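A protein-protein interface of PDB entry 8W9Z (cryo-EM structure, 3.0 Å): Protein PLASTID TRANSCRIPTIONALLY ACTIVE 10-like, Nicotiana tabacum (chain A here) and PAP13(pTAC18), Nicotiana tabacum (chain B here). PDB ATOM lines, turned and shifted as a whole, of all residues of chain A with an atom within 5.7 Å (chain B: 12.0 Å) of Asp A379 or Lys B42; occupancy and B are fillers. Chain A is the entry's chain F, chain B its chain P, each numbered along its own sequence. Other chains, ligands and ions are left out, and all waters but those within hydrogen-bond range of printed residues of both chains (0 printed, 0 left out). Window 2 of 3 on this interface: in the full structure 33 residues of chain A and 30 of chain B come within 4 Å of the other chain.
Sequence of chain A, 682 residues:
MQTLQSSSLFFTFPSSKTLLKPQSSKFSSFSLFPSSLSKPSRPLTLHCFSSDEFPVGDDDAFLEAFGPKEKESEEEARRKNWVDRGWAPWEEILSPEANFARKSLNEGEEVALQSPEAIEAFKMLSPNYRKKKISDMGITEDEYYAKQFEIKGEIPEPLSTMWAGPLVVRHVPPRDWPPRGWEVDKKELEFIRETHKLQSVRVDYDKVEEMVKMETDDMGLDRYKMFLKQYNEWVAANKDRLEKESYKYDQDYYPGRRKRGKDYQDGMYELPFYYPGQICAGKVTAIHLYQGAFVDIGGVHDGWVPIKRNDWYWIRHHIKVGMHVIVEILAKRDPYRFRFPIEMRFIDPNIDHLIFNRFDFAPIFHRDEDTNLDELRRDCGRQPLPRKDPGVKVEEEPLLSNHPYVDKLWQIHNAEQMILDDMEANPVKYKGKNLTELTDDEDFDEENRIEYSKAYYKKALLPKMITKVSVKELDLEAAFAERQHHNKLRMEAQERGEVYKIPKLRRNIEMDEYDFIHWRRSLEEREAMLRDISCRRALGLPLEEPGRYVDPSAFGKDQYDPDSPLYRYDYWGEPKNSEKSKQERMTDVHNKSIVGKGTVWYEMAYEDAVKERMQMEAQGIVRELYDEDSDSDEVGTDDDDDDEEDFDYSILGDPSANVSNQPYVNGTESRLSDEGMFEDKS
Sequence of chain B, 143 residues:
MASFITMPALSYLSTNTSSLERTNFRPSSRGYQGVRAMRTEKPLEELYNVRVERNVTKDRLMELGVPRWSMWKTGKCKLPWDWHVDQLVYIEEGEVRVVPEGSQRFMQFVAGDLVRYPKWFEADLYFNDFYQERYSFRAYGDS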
ATOM      1  N   ARG A 180      20.107 -40.334   6.163  1.00  0.00           N
ATOM      2  CA  ARG A 180      19.256 -39.160   6.023  1.00  0.00           C
ATOM      3  C   ARG A 180      19.672 -38.371   4.788  1.00  0.00           C
ATOM      4  O   ARG A 180      20.764 -37.793   4.749  1.00  0.00           O
ATOM      5  CB  ARG A 180      19.343 -38.289   7.273  1.00  0.00           C
ATOM      6  CG  ARG A 180      19.063 -39.030   8.570  1.00  0.00           C
ATOM      7  CD  ARG A 180      18.814 -38.067   9.723  1.00  0.00           C
ATOM      8  NE  ARG A 180      17.470 -37.495   9.682  1.00  0.00           N
ATOM      9  CZ  ARG A 180      17.170 -36.319   9.140  1.00  0.00           C
ATOM     10  NH1 ARG A 180      18.118 -35.577   8.587  1.00  0.00           N
ATOM     11  NH2 ARG A 180      15.916 -35.886   9.152  1.00  0.00           N
ATOM     12  N   ASP A 334      27.371 -41.187  15.452  1.00  0.00           N
ATOM     13  CA  ASP A 334      27.735 -40.287  14.363  1.00  0.00           C
ATOM     14  C   ASP A 334      29.214 -39.930  14.464  1.00  0.00           C
ATOM     15  O   ASP A 334      29.663 -39.470  15.519  1.00  0.00           O
ATOM     16  CB  ASP A 334      26.878 -39.025  14.414  1.00  0.00           C
ATOM     17  CG  ASP A 334      26.804 -38.308  13.079  1.00  0.00           C
ATOM     18  OD1 ASP A 334      27.858 -38.105  12.441  1.00  0.00           O
ATOM     19  OD2 ASP A 334      25.682 -37.946  12.664  1.00  0.00           O
ATOM     20  N   ARG A 337      30.151 -35.956  15.617  1.00  0.00           N
ATOM     21  CA  ARG A 337      30.111 -35.516  17.007  1.00  0.00           C
ATOM     22  C   ARG A 337      30.965 -36.409  17.901  1.00  0.00           C
ATOM     23  O   ARG A 337      31.777 -35.914  18.689  1.00  0.00           O
ATOM     24  CB  ARG A 337      28.664 -35.487  17.503  1.00  0.00           C
ATOM     25  CG  ARG A 337      28.507 -34.962  18.916  1.00  0.00           C
ATOM     26  CD  ARG A 337      29.103 -33.574  19.045  1.00  0.00           C
ATOM     27  NE  ARG A 337      28.432 -32.613  18.177  1.00  0.00           N
ATOM     28  CZ  ARG A 337      28.864 -31.376  17.961  1.00  0.00           C
ATOM     29  NH1 ARG A 337      29.971 -30.946  18.548  1.00  0.00           N
ATOM     30  NH2 ARG A 337      28.189 -30.569  17.154  1.00  0.00           N
ATOM     31  N   PHE A 338      30.794 -37.723  17.792  1.00  0.00           N
ATOM     32  CA  PHE A 338      31.490 -38.666  18.655  1.00  0.00           C
ATOM     33  C   PHE A 338      32.854 -39.021  18.081  1.00  0.00           C
ATOM     34  O   PHE A 338      33.014 -39.162  16.866  1.00  0.00           O
ATOM     35  CB  PHE A 338      30.655 -39.932  18.847  1.00  0.00           C
ATOM     36  CG  PHE A 338      29.359 -39.692  19.566  1.00  0.00           C
ATOM     37  CD1 PHE A 338      29.299 -39.749  20.946  1.00  0.00           C
ATOM     38  CD2 PHE A 338      28.205 -39.402  18.861  1.00  0.00           C
ATOM     39  CE1 PHE A 338      28.112 -39.526  21.610  1.00  0.00           C
ATOM     40  CE2 PHE A 338      27.015 -39.178  19.520  1.00  0.00           C
ATOM     41  CZ  PHE A 338      26.968 -39.240  20.896  1.00  0.00           C
ATOM     42  N   ASP A 374      23.457 -25.879  24.824  1.00  0.00           N
ATOM     43  CA  ASP A 374      22.219 -26.646  24.907  1.00  0.00           C
ATOM     44  C   ASP A 374      22.032 -27.528  23.678  1.00  0.00           C
ATOM     45  O   ASP A 374      21.613 -28.686  23.796  1.00  0.00           O
ATOM     46  CB  ASP A 374      21.030 -25.703  25.082  1.00  0.00           C
ATOM     47  CG  ASP A 374      19.768 -26.428  25.506  1.00  0.00           C
ATOM     48  OD1 ASP A 374      19.849 -27.634  25.825  1.00  0.00           O
ATOM     49  OD2 ASP A 374      18.692 -25.794  25.521  1.00  0.00           O
ATOM     50  N   GLU A 375      22.339 -27.002  22.489  1.00  0.00           N
ATOM     51  CA  GLU A 375      22.251 -27.816  21.282  1.00  0.00           C
ATOM     52  C   GLU A 375      23.225 -28.984  21.340  1.00  0.00           C
ATOM     53  O   GLU A 375      22.893 -30.102  20.932  1.00  0.00           O
ATOM     54  CB  GLU A 375      22.517 -26.959  20.045  1.00  0.00           C
ATOM     55  CG  GLU A 375      21.529 -25.825  19.842  1.00  0.00           C
ATOM     56  CD  GLU A 375      21.780 -25.060  18.559  1.00  0.00           C
ATOM     57  OE1 GLU A 375      22.633 -25.501  17.760  1.00  0.00           O
ATOM     58  OE2 GLU A 375      21.127 -24.018  18.348  1.00  0.00           O
ATOM     59  N   LEU A 376      24.433 -28.743  21.855  1.00  0.00           N
ATOM     60  CA  LEU A 376      25.400 -29.823  22.017  1.00  0.00           C
ATOM     61  C   LEU A 376      24.887 -30.878  22.989  1.00  0.00           C
ATOM     62  O   LEU A 376      25.009 -32.083  22.733  1.00  0.00           O
ATOM     63  CB  LEU A 376      26.736 -29.253  22.495  1.00  0.00           C
ATOM     64  CG  LEU A 376      27.890 -30.228  22.716  1.00  0.00           C
ATOM     65  CD1 LEU A 376      28.267 -30.905  21.413  1.00  0.00           C
ATOM     66  CD2 LEU A 376      29.087 -29.507  23.311  1.00  0.00           C
ATOM     67  N   ARG A 377      24.299 -30.442  24.106  1.00  0.00           N
ATOM     68  CA  ARG A 377      23.787 -31.387  25.093  1.00  0.00           C
ATOM     69  C   ARG A 377      22.640 -32.214  24.526  1.00  0.00           C
ATOM     70  O   ARG A 377      22.514 -33.405  24.830  1.00  0.00           O
ATOM     71  CB  ARG A 377      23.339 -30.642  26.349  1.00  0.00           C
ATOM     72  N   ARG A 378      21.791 -31.599  23.701  1.00  0.00           N
ATOM     73  CA  ARG A 378      20.670 -32.334  23.126  1.00  0.00           C
ATOM     74  C   ARG A 378      21.105 -33.234  21.977  1.00  0.00           C
ATOM     75  O   ARG A 378      20.443 -34.240  21.701  1.00  0.00           O
ATOM     76  CB  ARG A 378      19.585 -31.363  22.657  1.00  0.00           C
ATOM     77  CG  ARG A 378      19.046 -30.471  23.762  1.00  0.00           C
ATOM     78  CD  ARG A 378      17.900 -29.607  23.273  1.00  0.00           C
ATOM     79  NE  ARG A 378      16.611 -30.276  23.421  1.00  0.00           N
ATOM     80  CZ  ARG A 378      15.817 -30.131  24.475  1.00  0.00           C
ATOM     81  NH1 ARG A 378      16.178 -29.340  25.476  1.00  0.00           N
ATOM     82  NH2 ARG A 378      14.659 -30.776  24.531  1.00  0.00           N
ATOM     83  N   ASP A 379      22.200 -32.892  21.296  1.00  0.00           N
ATOM     84  CA  ASP A 379      22.700 -33.748  20.226  1.00  0.00           C
ATOM     85  C   ASP A 379      23.454 -34.951  20.780  1.00  0.00           C
ATOM     86  O   ASP A 379      23.358 -36.053  20.230  1.00  0.00           O
ATOM     87  CB  ASP A 379      23.600 -32.941  19.288  1.00  0.00           C
ATOM     88  CG  ASP A 379      23.925 -33.684  18.007  1.00  0.00           C
ATOM     89  OD1 ASP A 379      23.293 -34.727  17.740  1.00  0.00           O
ATOM     90  OD2 ASP A 379      24.817 -33.223  17.263  1.00  0.00           O
ATOM     91  N   CYS A 380      24.202 -34.761  21.868  1.00  0.00           N
ATOM     92  CA  CYS A 380      24.978 -35.863  22.429  1.00  0.00           C
ATOM     93  C   CYS A 380      24.122 -36.772  23.302  1.00  0.00           C
ATOM     94  O   CYS A 380      24.311 -37.993  23.301  1.00  0.00           O
ATOM     95  CB  CYS A 380      26.159 -35.315  23.226  1.00  0.00           C
ATOM     96  SG  CYS A 380      27.252 -34.250  22.265  1.00  0.00           S
ATOM     97  N   GLY A 381      23.184 -36.202  24.048  1.00  0.00           N
ATOM     98  CA  GLY A 381      22.346 -36.970  24.940  1.00  0.00           C
ATOM     99  C   GLY A 381      22.702 -36.881  26.406  1.00  0.00           C
ATOM    100  O   GLY A 381      22.303 -37.763  27.173  1.00  0.00           O
ATOM    101  N   MET B  38      29.222 -27.710   9.061  1.00  0.00           N
ATOM    102  CA  MET B  38      28.708 -29.051   8.808  1.00  0.00           C
ATOM    103  C   MET B  38      27.522 -29.013   7.853  1.00  0.00           C
ATOM    104  O   MET B  38      26.714 -28.085   7.895  1.00  0.00           O
ATOM    105  CB  MET B  38      28.299 -29.726  10.121  1.00  0.00           C
ATOM    106  CG  MET B  38      27.772 -31.144   9.949  1.00  0.00           C
ATOM    107  SD  MET B  38      26.981 -31.803  11.428  1.00  0.00           S
ATOM    108  CE  MET B  38      26.550 -33.450  10.873  1.00  0.00           C
ATOM    109  N   ARG B  39      27.424 -30.022   6.986  1.00  0.00           N
ATOM    110  CA  ARG B  39      26.239 -30.218   6.153  1.00  0.00           C
ATOM    111  C   ARG B  39      25.151 -30.797   7.051  1.00  0.00           C
ATOM    112  O   ARG B  39      24.951 -32.010   7.150  1.00  0.00           O
ATOM    113  CB  ARG B  39      26.543 -31.129   4.971  1.00  0.00           C
ATOM    114  CG  ARG B  39      27.752 -30.705   4.150  1.00  0.00           C
ATOM    115  CD  ARG B  39      27.602 -29.286   3.623  1.00  0.00           C
ATOM    116  NE  ARG B  39      28.747 -28.890   2.809  1.00  0.00           N
ATOM    117  CZ  ARG B  39      29.832 -28.291   3.287  1.00  0.00           C
ATOM    118  NH1 ARG B  39      29.925 -28.015   4.581  1.00  0.00           N
ATOM    119  NH2 ARG B  39      30.827 -27.969   2.471  1.00  0.00           N
ATOM    120  N   THR B  40      24.439 -29.901   7.731  1.00  0.00           N
ATOM    121  CA  THR B  40      23.513 -30.282   8.791  1.00  0.00           C
ATOM    122  C   THR B  40      22.335 -31.095   8.271  1.00  0.00           C
ATOM    123  O   THR B  40      21.477 -30.574   7.551  1.00  0.00           O
ATOM    124  CB  THR B  40      22.997 -29.037   9.519  1.00  0.00           C
ATOM    125  OG1 THR B  40      24.105 -28.303  10.057  1.00  0.00           O
ATOM    126  CG2 THR B  40      22.061 -29.431  10.650  1.00  0.00           C
ATOM    127  N   GLU B  41      22.290 -32.378   8.633  1.00  0.00           N
ATOM    128  CA  GLU B  41      21.109 -33.209   8.452  1.00  0.00           C
ATOM    129  C   GLU B  41      20.310 -33.343   9.744  1.00  0.00           C
ATOM    130  O   GLU B  41      19.474 -34.245   9.862  1.00  0.00           O
ATOM    131  CB  GLU B  41      21.498 -34.592   7.928  1.00  0.00           C
ATOM    132  CG  GLU B  41      22.109 -34.591   6.535  1.00  0.00           C
ATOM    133  CD  GLU B  41      23.624 -34.643   6.561  1.00  0.00           C
ATOM    134  OE1 GLU B  41      24.198 -34.773   7.663  1.00  0.00           O
ATOM    135  OE2 GLU B  41      24.241 -34.554   5.479  1.00  0.00           O
ATOM    136  N   LYS B  42      20.556 -32.459  10.714  1.00  0.00           N
ATOM    137  CA  LYS B  42      19.917 -32.492  12.027  1.00  0.00           C
ATOM    138  C   LYS B  42      19.203 -31.161  12.236  1.00  0.00           C
ATOM    139  O   LYS B  42      19.727 -30.264  12.915  1.00  0.00           O
ATOM    140  CB  LYS B  42      20.942 -32.752  13.130  1.00  0.00           C
ATOM    141  CG  LYS B  42      20.358 -33.262  14.437  1.00  0.00           C
ATOM    142  CD  LYS B  42      19.929 -34.716  14.318  1.00  0.00           C
ATOM    143  CE  LYS B  42      21.104 -35.611  13.959  1.00  0.00           C
ATOM    144  NZ  LYS B  42      22.182 -35.550  14.985  1.00  0.00           N
ATOM    145  N   PRO B  43      18.013 -30.993  11.664  1.00  0.00           N
ATOM    146  CA  PRO B  43      17.296 -29.723  11.816  1.00  0.00           C
ATOM    147  C   PRO B  43      16.811 -29.513  13.242  1.00  0.00           C
ATOM    148  O   PRO B  43      16.735 -30.439  14.051  1.00  0.00           O
ATOM    149  CB  PRO B  43      16.119 -29.862  10.845  1.00  0.00           C
ATOM    150  CG  PRO B  43      15.906 -31.333  10.733  1.00  0.00           C
ATOM    151  CD  PRO B  43      17.273 -31.949  10.825  1.00  0.00           C
ATOM    152  N   LEU B  44      16.474 -28.259  13.542  1.00  0.00           N
ATOM    153  CA  LEU B  44      16.005 -27.896  14.872  1.00  0.00           C
ATOM    154  C   LEU B  44      14.565 -28.314  15.132  1.00  0.00           C
ATOM    155  O   LEU B  44      14.101 -28.190  16.270  1.00  0.00           O
ATOM    156  CB  LEU B  44      16.142 -26.387  15.085  1.00  0.00           C
ATOM    157  CG  LEU B  44      17.565 -25.834  15.161  1.00  0.00           C
ATOM    158  CD1 LEU B  44      17.538 -24.327  15.326  1.00  0.00           C
ATOM    159  CD2 LEU B  44      18.329 -26.485  16.301  1.00  0.00           C
ATOM    160  N   GLU B  45      13.851 -28.805  14.118  1.00  0.00           N
ATOM    161  CA  GLU B  45      12.481 -29.253  14.338  1.00  0.00           C
ATOM    162  C   GLU B  45      12.437 -30.565  15.111  1.00  0.00           C
ATOM    163  O   GLU B  45      11.437 -30.854  15.779  1.00  0.00           O
ATOM    164  CB  GLU B  45      11.753 -29.398  13.001  1.00  0.00           C
ATOM    165  CG  GLU B  45      11.700 -28.123  12.173  1.00  0.00           C
ATOM    166  CD  GLU B  45      10.781 -27.069  12.764  1.00  0.00           C
ATOM    167  OE1 GLU B  45       9.993 -27.398  13.676  1.00  0.00           O
ATOM    168  OE2 GLU B  45      10.845 -25.908  12.310  1.00  0.00           O
ATOM    169  N   GLU B  46      13.500 -31.369  15.034  1.00  0.00           N
ATOM    170  CA  GLU B  46      13.568 -32.625  15.765  1.00  0.00           C
ATOM    171  C   GLU B  46      14.646 -32.650  16.838  1.00  0.00           C
ATOM    172  O   GLU B  46      14.561 -33.476  17.750  1.00  0.00           O
ATOM    173  CB  GLU B  46      13.788 -33.798  14.797  1.00  0.00           C
ATOM    174  CG  GLU B  46      14.871 -33.570  13.759  1.00  0.00           C
ATOM    175  CD  GLU B  46      16.264 -33.812  14.302  1.00  0.00           C
ATOM    176  OE1 GLU B  46      16.405 -34.608  15.254  1.00  0.00           O
ATOM    177  OE2 GLU B  46      17.216 -33.203  13.777  1.00  0.00           O
ATOM    178  N   LEU B  47      15.655 -31.782  16.750  1.00  0.00           N
ATOM    179  CA  LEU B  47      16.593 -31.624  17.856  1.00  0.00           C
ATOM    180  C   LEU B  47      15.863 -31.132  19.099  1.00  0.00           C
ATOM    181  O   LEU B  47      15.869 -31.790  20.146  1.00  0.00           O
ATOM    182  CB  LEU B  47      17.714 -30.664  17.458  1.00  0.00           C
ATOM    183  CG  LEU B  47      18.872 -30.524  18.448  1.00  0.00           C
ATOM    184  CD1 LEU B  47      19.509 -31.875  18.721  1.00  0.00           C
ATOM    185  CD2 LEU B  47      19.902 -29.541  17.920  1.00  0.00           C
ATOM    186  N   TYR B  48      15.226 -29.968  18.997  1.00  0.00           N
ATOM    187  CA  TYR B  48      14.194 -29.584  19.948  1.00  0.00           C
ATOM    188  C   TYR B  48      12.877 -30.200  19.493  1.00  0.00           C
ATOM    189  O   TYR B  48      12.489 -30.056  18.330  1.00  0.00           O
ATOM    190  CB  TYR B  48      14.069 -28.063  20.033  1.00  0.00           C
ATOM    191  CG  TYR B  48      15.324 -27.353  20.480  1.00  0.00           C
ATOM    192  CD1 TYR B  48      15.573 -27.124  21.826  1.00  0.00           C
ATOM    193  CD2 TYR B  48      16.252 -26.897  19.556  1.00  0.00           C
ATOM    194  CE1 TYR B  48      16.715 -26.467  22.238  1.00  0.00           C
ATOM    195  CE2 TYR B  48      17.398 -26.242  19.959  1.00  0.00           C
ATOM    196  CZ  TYR B  48      17.624 -26.030  21.301  1.00  0.00           C
ATOM    197  OH  TYR B  48      18.764 -25.376  21.707  1.00  0.00           O
ATOM    198  N   ASN B  49      12.191 -30.885  20.406  1.00  0.00           N
ATOM    199  CA  ASN B  49      11.024 -31.686  20.036  1.00  0.00           C
ATOM    200  C   ASN B  49       9.858 -30.758  19.708  1.00  0.00           C
ATOM    201  O   ASN B  49       8.919 -30.575  20.485  1.00  0.00           O
ATOM    202  CB  ASN B  49      10.666 -32.661  21.151  1.00  0.00           C
ATOM    203  CG  ASN B  49       9.563 -33.616  20.752  1.00  0.00           C
ATOM    204  OD1 ASN B  49       8.422 -33.484  21.190  1.00  0.00           O
ATOM    205  ND2 ASN B  49       9.897 -34.581  19.904  1.00  0.00           N
ATOM    206  N   VAL B  50       9.923 -30.167  18.521  1.00  0.00           N
ATOM    207  CA  VAL B  50       8.887 -29.266  18.020  1.00  0.00           C
ATOM    208  C   VAL B  50       8.316 -29.920  16.768  1.00  0.00           C
ATOM    209  O   VAL B  50       8.821 -29.733  15.657  1.00  0.00           O
ATOM    210  CB  VAL B  50       9.425 -27.864  17.728  1.00  0.00           C
ATOM    211  CG1 VAL B  50       8.300 -26.942  17.299  1.00  0.00           C
ATOM    212  CG2 VAL B  50      10.141 -27.305  18.947  1.00  0.00           C
ATOM    213  N   VAL B  52       6.121 -30.329  13.715  1.00  0.00           N
ATOM    214  CA  VAL B  52       5.440 -29.412  12.811  1.00  0.00           C
ATOM    215  C   VAL B  52       4.841 -30.213  11.662  1.00  0.00           C
ATOM    216  O   VAL B  52       5.545 -30.981  10.997  1.00  0.00           O
ATOM    217  CB  VAL B  52       6.392 -28.319  12.286  1.00  0.00           C
ATOM    218  CG1 VAL B  52       7.723 -28.923  11.859  1.00  0.00           C
ATOM    219  CG2 VAL B  52       5.750 -27.560  11.136  1.00  0.00           C
ATOM    220  N   ARG B  54       3.111 -29.647   8.125  1.00  0.00           N
ATOM    221  CA  ARG B  54       2.937 -28.636   7.092  1.00  0.00           C
ATOM    222  C   ARG B  54       1.812 -29.028   6.143  1.00  0.00           C
ATOM    223  O   ARG B  54       1.666 -30.201   5.786  1.00  0.00           O
ATOM    224  CB  ARG B  54       4.238 -28.434   6.314  1.00  0.00           C
ATOM    225  CG  ARG B  54       5.377 -27.890   7.161  1.00  0.00           C
ATOM    226  CD  ARG B  54       6.623 -27.640   6.329  1.00  0.00           C
ATOM    227  NE  ARG B  54       7.679 -27.008   7.113  1.00  0.00           N
ATOM    228  CZ  ARG B  54       8.592 -27.674   7.811  1.00  0.00           C
ATOM    229  NH1 ARG B  54       8.582 -29.000   7.825  1.00  0.00           N
ATOM    230  NH2 ARG B  54       9.517 -27.015   8.496  1.00  0.00           N
ATOM    231  N   PRO B 100      15.456 -20.561  19.930  1.00  0.00           N
ATOM    232  CA  PRO B 100      15.689 -21.099  21.276  1.00  0.00           C
ATOM    233  C   PRO B 100      16.722 -20.281  22.038  1.00  0.00           C
ATOM    234  O   PRO B 100      17.446 -19.451  21.483  1.00  0.00           O
ATOM    235  CB  PRO B 100      16.185 -22.523  21.007  1.00  0.00           C
ATOM    236  CG  PRO B 100      15.629 -22.864  19.664  1.00  0.00           C
ATOM    237  CD  PRO B 100      15.650 -21.581  18.887  1.00  0.00           C
ATOM    238  N   SER B 103      20.723 -19.734  21.211  1.00  0.00           N
ATOM    239  CA  SER B 103      20.985 -20.265  19.883  1.00  0.00           C
ATOM    240  C   SER B 103      21.090 -19.140  18.861  1.00  0.00           C
ATOM    241  O   SER B 103      20.570 -18.039  19.053  1.00  0.00           O
ATOM    242  CB  SER B 103      19.885 -21.243  19.466  1.00  0.00           C
ATOM    243  OG  SER B 103      18.629 -20.591  19.404  1.00  0.00           O
ATOM    244  N   GLN B 104      21.781 -19.437  17.761  1.00  0.00           N
ATOM    245  CA  GLN B 104      21.901 -18.515  16.645  1.00  0.00           C
ATOM    246  C   GLN B 104      21.155 -18.979  15.403  1.00  0.00           C
ATOM    247  O   GLN B 104      21.070 -18.219  14.432  1.00  0.00           O
ATOM    248  CB  GLN B 104      23.379 -18.287  16.289  1.00  0.00           C
ATOM    249  CG  GLN B 104      24.144 -17.433  17.291  1.00  0.00           C
ATOM    250  CD  GLN B 104      24.480 -18.177  18.569  1.00  0.00           C
ATOM    251  OE1 GLN B 104      24.564 -17.582  19.644  1.00  0.00           O
ATOM    252  NE2 GLN B 104      24.683 -19.486  18.457  1.00  0.00           N
ATOM    253  N   ARG B 105      20.617 -20.194  15.407  1.00  0.00           N
ATOM    254  CA  ARG B 105      19.820 -20.711  14.305  1.00  0.00           C
ATOM    255  C   ARG B 105      18.355 -20.757  14.717  1.00  0.00           C
ATOM    256  O   ARG B 105      18.032 -21.111  15.855  1.00  0.00           O
ATOM    257  CB  ARG B 105      20.297 -22.102  13.880  1.00  0.00           C
ATOM    258  CG  ARG B 105      21.780 -22.161  13.542  1.00  0.00           C
ATOM    259  CD  ARG B 105      22.136 -23.393  12.722  1.00  0.00           C
ATOM    260  NE  ARG B 105      21.833 -24.643  13.414  1.00  0.00           N
ATOM    261  CZ  ARG B 105      20.798 -25.425  13.126  1.00  0.00           C
ATOM    262  NH1 ARG B 105      19.963 -25.089  12.153  1.00  0.00           N
ATOM    263  NH2 ARG B 105      20.601 -26.544  13.807  1.00  0.00           N
ATOM    264  N   PHE B 106      17.475 -20.393  13.791  1.00  0.00           N
ATOM    265  CA  PHE B 106      16.051 -20.288  14.057  1.00  0.00           C
ATOM    266  C   PHE B 106      15.274 -21.268  13.188  1.00  0.00           C
ATOM    267  O   PHE B 106      15.796 -21.824  12.218  1.00  0.00           O
ATOM    268  CB  PHE B 106      15.545 -18.860  13.807  1.00  0.00           C
ATOM    269  CG  PHE B 106      15.874 -18.330  12.438  1.00  0.00           C
ATOM    270  CD1 PHE B 106      17.057 -17.646  12.212  1.00  0.00           C
ATOM    271  CD2 PHE B 106      14.997 -18.511  11.380  1.00  0.00           C
ATOM    272  CE1 PHE B 106      17.361 -17.157  10.956  1.00  0.00           C
ATOM    273  CE2 PHE B 106      15.298 -18.024  10.123  1.00  0.00           C
ATOM    274  CZ  PHE B 106      16.481 -17.347   9.912  1.00  0.00           C
ATOM    275  N   MET B 107      14.012 -21.470  13.552  1.00  0.00           N
ATOM    276  CA  MET B 107      13.089 -22.301  12.791  1.00  0.00           C
ATOM    277  C   MET B 107      11.891 -21.459  12.378  1.00  0.00           C
ATOM    278  O   MET B 107      11.321 -20.735  13.201  1.00  0.00           O
ATOM    279  CB  MET B 107      12.643 -23.521  13.602  1.00  0.00           C
ATOM    280  CG  MET B 107      12.300 -23.226  15.052  1.00  0.00           C
ATOM    281  SD  MET B 107      11.929 -24.731  15.973  1.00  0.00           S
ATOM    282  CE  MET B 107      11.717 -24.078  17.625  1.00  0.00           C
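The side-chain hydroxyl (OG) of Ser B103 lies within hydrogen-bond range of the backbone carbonyl oxygen (O) of Pro B100 (2.6 Å). The guanidinium group (NE) of Arg A337 lies within salt-bridge range of the side-chain carboxylate (OD2) of Asp A379 (3.8 Å).
Among the printed residues, pairs that only touch across the chains: Asp A374 with Tyr B48, Glu A375 with Tyr B48, Glu A375 with Ser B103, Arg A378 with Leu B47, Arg A378 with Tyr B48 and Asp A379 with Leu B47.
The side-chain carboxylate of Asp A379 is in salt-bridge range of the side-chain amino group of Lys B42 (3.1 Å). The guanidinium group (NH1) of Arg A180 lies close to the backbone carbonyl oxygen (O) of Glu B41 (2.3 Å).
Among the printed residues, 8 pairs touch across the chains.
No residue of chain B comes within 4 Å of Arg A337. Of the printed residues of chain B, Asp A374 touches Tyr B48 (3.8 Å). Printed residues of chain B within 4 Å of Glu A375: Tyr B48 and Ser B103. No residue of chain B comes within 4 Å of Leu A376. Asp A379 touches just these residues of chain B: Lys B42 (3.1 Å) and Leu B47 (3.9 Å). No residue of chain B comes within 4 Å of Gly A381. Of the printed residues of chain A, Glu B41 touches Arg A180. Lys B42 touches just one residue of chain A: Asp A379. Of the printed residues of chain A, Tyr B48 touches Asp A374, Glu A375 and Arg A378. Of the printed residues of chain A, Ser B103 touches Glu A375. The nearest residue of chain B that does not touch Asp A379 is Met B38 (6.4 Å). The nearest printed residue of chain B that does not touch Arg A378 is Asn B49 (4.8 Å).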
